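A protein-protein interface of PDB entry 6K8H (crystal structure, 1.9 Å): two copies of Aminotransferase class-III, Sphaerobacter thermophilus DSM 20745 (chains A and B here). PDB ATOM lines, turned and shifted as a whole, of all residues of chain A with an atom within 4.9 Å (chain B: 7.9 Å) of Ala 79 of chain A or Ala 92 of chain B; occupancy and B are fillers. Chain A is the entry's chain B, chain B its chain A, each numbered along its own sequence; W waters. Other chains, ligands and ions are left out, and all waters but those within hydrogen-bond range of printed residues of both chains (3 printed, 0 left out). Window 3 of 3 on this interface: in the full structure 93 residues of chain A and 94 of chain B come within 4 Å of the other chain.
The backbone carbonyl oxygen (O) of Leu 91 of chain B is in hydrogen-bond range of the side-chain amide nitrogen (ND2) of Asn 84 of chain A. N of Gly 51 of chain A lies within hydrogen-bond range of O of Asp 93 of chain B (2.8 Å).
CE2 of Phe 97 of chain B touches N of Gly 51 of chain A, at 3.8 Å. Phe 97 of chain B touches His 78 of chain A (CD2 to CE1, 3.6 Å). Leu 91 of chain B touches Ala 79 of chain A. Ala 92 of chain B touches Ala 79 of chain A.
Gly 77 of chain A touches none of the printed residues of chain B. Of the printed residues of chain B, His 78 of chain A touches Phe 97 (3.6 Å). Of chain B, only Leu 91 and Ala 92 come within 4 Å of Ala 79 of chain A. Of the printed residues of chain B, Asn 84 of chain A touches Leu 91. Ala 86 of chain B touches none of the printed residues of chain A. Printed residues of chain A within 4 Å of Leu 91 of chain B: Ala 79 (3.6 Å) and Asn 84 (2.9 Å). Ala 92 of chain B touches one residue of chain A. Of the printed residues of chain A, Phe 97 of chain B touches Gly 51 (3.8 Å) and His 78 (3.6 Å).
Printed residues of chain B that touch a printed residue of chain A: Leu 91, Ala 92, Asp 93 and Phe 97. Of the 7 printed residues of chain A, 4 touch a printed residue of chain B. Printed residues of chain A that touch a printed residue of chain B: Gly 51, His 78, Ala 79 and Asn 84. Hydrophobic or aromatic side chains of chain A that line the printed part of chain B: His 78 and Ala 79. Among the printed residues, no Asp or Glu carboxylate lies within 4 Å of a Lys or Arg side-chain nitrogen of the other chain.
No position is printed for both chains. Of the 6 pairs that touch across the chains among the printed residues, none has its exchanged pair printed and touching as well.
Water W3 bridges O of Gly 51 of chain A and O of Ala 92 of chain B. Water W2 lies within hydrogen-bond range of ND1 of His 78 of chain A (2.9 Å), O of Ala 96 of chain B (3.0 Å) and N of Val 95 of chain B (3.2 Å). Water W1 lies within hydrogen-bond range of the backbone NH of Ala 79 of chain A (3.0 Å) and the backbone NH of Val 95 of chain B (3.1 Å).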
ATOM      1  N   GLY A  51      16.429  16.808 -13.987  1.00  0.00           N
ATOM      2  CA  GLY A  51      16.148  18.230 -13.998  1.00  0.00           C
ATOM      3  C   GLY A  51      15.091  18.558 -15.028  1.00  0.00           C
ATOM      4  O   GLY A  51      14.857  17.806 -15.981  1.00  0.00           O
ATOM      5  N   GLY A  77      19.173  25.591 -19.205  1.00  0.00           N
ATOM      6  CA  GLY A  77      18.623  24.783 -18.130  1.00  0.00           C
ATOM      7  C   GLY A  77      18.550  23.315 -18.499  1.00  0.00           C
ATOM      8  O   GLY A  77      19.199  22.855 -19.429  1.00  0.00           O
ATOM      9  N   HIS A  78      17.719  22.577 -17.764  1.00  0.00           N
ATOM     10  CA  HIS A  78      17.702  21.120 -17.853  1.00  0.00           C
ATOM     11  C   HIS A  78      16.696  20.626 -18.881  1.00  0.00           C
ATOM     12  O   HIS A  78      15.572  21.129 -18.959  1.00  0.00           O
ATOM     13  CB  HIS A  78      17.362  20.492 -16.500  1.00  0.00           C
ATOM     14  CG  HIS A  78      18.365  20.780 -15.432  1.00  0.00           C
ATOM     15  ND1 HIS A  78      19.543  20.074 -15.303  1.00  0.00           N
ATOM     16  CD2 HIS A  78      18.379  21.720 -14.460  1.00  0.00           C
ATOM     17  CE1 HIS A  78      20.231  20.556 -14.286  1.00  0.00           C
ATOM     18  NE2 HIS A  78      19.546  21.550 -13.753  1.00  0.00           N
ATOM     19  N   ALA A  79      17.109  19.620 -19.655  1.00  0.00           N
ATOM     20  CA  ALA A  79      16.233  18.931 -20.604  1.00  0.00           C
ATOM     21  C   ALA A  79      15.488  19.918 -21.502  1.00  0.00           C
ATOM     22  O   ALA A  79      14.265  19.853 -21.669  1.00  0.00           O
ATOM     23  CB  ALA A  79      15.246  18.015 -19.876  1.00  0.00           C
ATOM     24  N   ASP A  80      16.242  20.831 -22.094  1.00  0.00           N
ATOM     25  CA  ASP A  80      15.642  21.770 -23.023  1.00  0.00           C
ATOM     26  C   ASP A  80      15.039  21.001 -24.194  1.00  0.00           C
ATOM     27  O   ASP A  80      15.730  20.167 -24.797  1.00  0.00           O
ATOM     28  CB  ASP A  80      16.672  22.772 -23.528  1.00  0.00           C
ATOM     29  CG  ASP A  80      16.110  23.669 -24.614  1.00  0.00           C
ATOM     30  OD1 ASP A  80      15.527  24.716 -24.277  1.00  0.00           O
ATOM     31  OD2 ASP A  80      16.234  23.314 -25.802  1.00  0.00           O
ATOM     32  N   PRO A  81      13.770  21.244 -24.545  1.00  0.00           N
ATOM     33  CA  PRO A  81      13.126  20.411 -25.577  1.00  0.00           C
ATOM     34  C   PRO A  81      13.695  20.606 -26.969  1.00  0.00           C
ATOM     35  O   PRO A  81      13.767  19.636 -27.730  1.00  0.00           O
ATOM     36  CB  PRO A  81      11.648  20.840 -25.520  1.00  0.00           C
ATOM     37  CG  PRO A  81      11.509  21.715 -24.341  1.00  0.00           C
ATOM     38  CD  PRO A  81      12.854  22.264 -24.004  1.00  0.00           C
ATOM     39  N   ASN A  84      16.942  18.742 -27.215  1.00  0.00           N
ATOM     40  CA  ASN A  84      16.661  17.305 -27.206  1.00  0.00           C
ATOM     41  C   ASN A  84      16.105  16.827 -28.544  1.00  0.00           C
ATOM     42  O   ASN A  84      16.510  15.772 -29.045  1.00  0.00           O
ATOM     43  CB  ASN A  84      15.703  16.952 -26.063  1.00  0.00           C
ATOM     44  CG  ASN A  84      16.429  16.810 -24.725  1.00  0.00           C
ATOM     45  OD1 ASN A  84      17.656  16.922 -24.665  1.00  0.00           O
ATOM     46  ND2 ASN A  84      15.677  16.572 -23.655  1.00  0.00           N
ATOM     47  N   ALA B  86      18.756   4.119 -24.811  1.00  0.00           N
ATOM     48  CA  ALA B  86      19.260   4.542 -23.512  1.00  0.00           C
ATOM     49  C   ALA B  86      19.508   6.048 -23.471  1.00  0.00           C
ATOM     50  O   ALA B  86      19.150   6.729 -22.498  1.00  0.00           O
ATOM     51  CB  ALA B  86      20.528   3.757 -23.189  1.00  0.00           C
ATOM     52  N   VAL B  87      20.107   6.589 -24.529  1.00  0.00           N
ATOM     53  CA  VAL B  87      20.367   8.023 -24.586  1.00  0.00           C
ATOM     54  C   VAL B  87      19.062   8.813 -24.591  1.00  0.00           C
ATOM     55  O   VAL B  87      18.938   9.831 -23.905  1.00  0.00           O
ATOM     56  CB  VAL B  87      21.247   8.351 -25.809  1.00  0.00           C
ATOM     57  CG1 VAL B  87      21.277   9.838 -26.056  1.00  0.00           C
ATOM     58  CG2 VAL B  87      22.664   7.846 -25.571  1.00  0.00           C
ATOM     59  N   ILE B  88      18.084   8.357 -25.371  1.00  0.00           N
ATOM     60  CA  ILE B  88      16.783   9.087 -25.455  1.00  0.00           C
ATOM     61  C   ILE B  88      16.133   9.091 -24.068  1.00  0.00           C
ATOM     62  O   ILE B  88      15.623  10.131 -23.660  1.00  0.00           O
ATOM     63  CB  ILE B  88      15.885   8.498 -26.555  1.00  0.00           C
ATOM     64  CG1 ILE B  88      16.437   8.826 -27.945  1.00  0.00           C
ATOM     65  CG2 ILE B  88      14.456   8.980 -26.389  1.00  0.00           C
ATOM     66  CD1 ILE B  88      15.901   7.963 -29.046  1.00  0.00           C
ATOM     67  N   ARG B  89      16.191   7.962 -23.368  1.00  0.00           N
ATOM     68  CA  ARG B  89      15.681   7.912 -22.001  1.00  0.00           C
ATOM     69  C   ARG B  89      16.370   8.954 -21.127  1.00  0.00           C
ATOM     70  O   ARG B  89      15.710   9.668 -20.357  1.00  0.00           O
ATOM     71  CB  ARG B  89      15.877   6.505 -21.437  1.00  0.00           C
ATOM     72  CG  ARG B  89      15.092   6.183 -20.192  1.00  0.00           C
ATOM     73  CD  ARG B  89      14.951   4.666 -20.003  1.00  0.00           C
ATOM     74  NE  ARG B  89      16.236   3.986 -19.818  1.00  0.00           N
ATOM     75  CZ  ARG B  89      16.798   3.171 -20.710  1.00  0.00           C
ATOM     76  NH1 ARG B  89      16.191   2.925 -21.869  1.00  0.00           N
ATOM     77  NH2 ARG B  89      17.974   2.606 -20.448  1.00  0.00           N
ATOM     78  N   GLN B  90      17.701   9.079 -21.256  1.00  0.00           N
ATOM     79  CA  GLN B  90      18.423  10.028 -20.410  1.00  0.00           C
ATOM     80  C   GLN B  90      18.114  11.475 -20.772  1.00  0.00           C
ATOM     81  O   GLN B  90      18.133  12.347 -19.895  1.00  0.00           O
ATOM     82  CB  GLN B  90      19.931   9.797 -20.494  1.00  0.00           C
ATOM     83  CG  GLN B  90      20.721  10.711 -19.584  1.00  0.00           C
ATOM     84  CD  GLN B  90      20.321  10.560 -18.131  1.00  0.00           C
ATOM     85  OE1 GLN B  90      20.150   9.438 -17.640  1.00  0.00           O
ATOM     86  NE2 GLN B  90      20.168  11.692 -17.429  1.00  0.00           N
ATOM     87  N   LEU B  91      17.877  11.760 -22.053  1.00  0.00           N
ATOM     88  CA  LEU B  91      17.657  13.146 -22.460  1.00  0.00           C
ATOM     89  C   LEU B  91      16.485  13.765 -21.711  1.00  0.00           C
ATOM     90  O   LEU B  91      16.512  14.959 -21.389  1.00  0.00           O
ATOM     91  CB  LEU B  91      17.411  13.240 -23.969  1.00  0.00           C
ATOM     92  CG  LEU B  91      18.494  12.841 -24.983  1.00  0.00           C
ATOM     93  CD1 LEU B  91      17.973  12.995 -26.409  1.00  0.00           C
ATOM     94  CD2 LEU B  91      19.759  13.661 -24.821  1.00  0.00           C
ATOM     95  N   ALA B  92      15.452  12.970 -21.427  1.00  0.00           N
ATOM     96  CA  ALA B  92      14.290  13.472 -20.703  1.00  0.00           C
ATOM     97  C   ALA B  92      14.629  13.904 -19.281  1.00  0.00           C
ATOM     98  O   ALA B  92      13.933  14.764 -18.726  1.00  0.00           O
ATOM     99  CB  ALA B  92      13.194  12.412 -20.696  1.00  0.00           C
ATOM    100  N   ASP B  93      15.704  13.361 -18.701  1.00  0.00           N
ATOM    101  CA  ASP B  93      16.128  13.693 -17.342  1.00  0.00           C
ATOM    102  C   ASP B  93      17.139  14.829 -17.283  1.00  0.00           C
ATOM    103  O   ASP B  93      17.305  15.427 -16.213  1.00  0.00           O
ATOM    104  CB  ASP B  93      16.779  12.483 -16.669  1.00  0.00           C
ATOM    105  CG  ASP B  93      15.775  11.438 -16.218  1.00  0.00           C
ATOM    106  OD1 ASP B  93      14.550  11.691 -16.305  1.00  0.00           O
ATOM    107  OD2 ASP B  93      16.231  10.358 -15.771  1.00  0.00           O
ATOM    108  N   GLY B  94      17.819  15.127 -18.384  1.00  0.00           N
ATOM    109  CA  GLY B  94      18.894  16.097 -18.458  1.00  0.00           C
ATOM    110  C   GLY B  94      20.235  15.439 -18.769  1.00  0.00           C
ATOM    111  O   GLY B  94      20.478  14.269 -18.448  1.00  0.00           O
ATOM    112  N   VAL B  95      21.128  16.210 -19.387  1.00  0.00           N
ATOM    113  CA  VAL B  95      22.347  15.643 -19.957  1.00  0.00           C
ATOM    114  C   VAL B  95      23.601  15.961 -19.157  1.00  0.00           C
ATOM    115  O   VAL B  95      24.647  15.341 -19.418  1.00  0.00           O
ATOM    116  CB  VAL B  95      22.534  16.065 -21.433  1.00  0.00           C
ATOM    117  CG1 VAL B  95      21.309  15.667 -22.253  1.00  0.00           C
ATOM    118  CG2 VAL B  95      22.799  17.578 -21.556  1.00  0.00           C
ATOM    119  N   ALA B  96      23.543  16.881 -18.197  1.00  0.00           N
ATOM    120  CA  ALA B  96      24.718  17.231 -17.400  1.00  0.00           C
ATOM    121  C   ALA B  96      24.268  17.970 -16.148  1.00  0.00           C
ATOM    122  O   ALA B  96      23.313  18.749 -16.200  1.00  0.00           O
ATOM    123  CB  ALA B  96      25.700  18.104 -18.191  1.00  0.00           C
ATOM    124  N   PHE B  97      24.971  17.734 -15.037  1.00  0.00           N
ATOM    125  CA  PHE B  97      24.603  18.283 -13.737  1.00  0.00           C
ATOM    126  C   PHE B  97      25.854  18.647 -12.948  1.00  0.00           C
ATOM    127  O   PHE B  97      26.872  17.959 -13.039  1.00  0.00           O
ATOM    128  CB  PHE B  97      23.801  17.277 -12.895  1.00  0.00           C
ATOM    129  CG  PHE B  97      22.603  16.711 -13.589  1.00  0.00           C
ATOM    130  CD1 PHE B  97      22.716  15.601 -14.404  1.00  0.00           C
ATOM    131  CD2 PHE B  97      21.346  17.286 -13.412  1.00  0.00           C
ATOM    132  CE1 PHE B  97      21.602  15.071 -15.039  1.00  0.00           C
ATOM    133  CE2 PHE B  97      20.238  16.760 -14.047  1.00  0.00           C
ATOM    134  CZ  PHE B  97      20.365  15.650 -14.858  1.00  0.00           C
HETATM  135  O   HOH W   1      19.969  18.967 -20.094  1.00  0.00           O
HETATM  136  O   HOH W   2      20.687  18.766 -17.584  1.00  0.00           O
HETATM  137  O   HOH W   3      13.240  15.554 -15.952  1.00  0.00           O
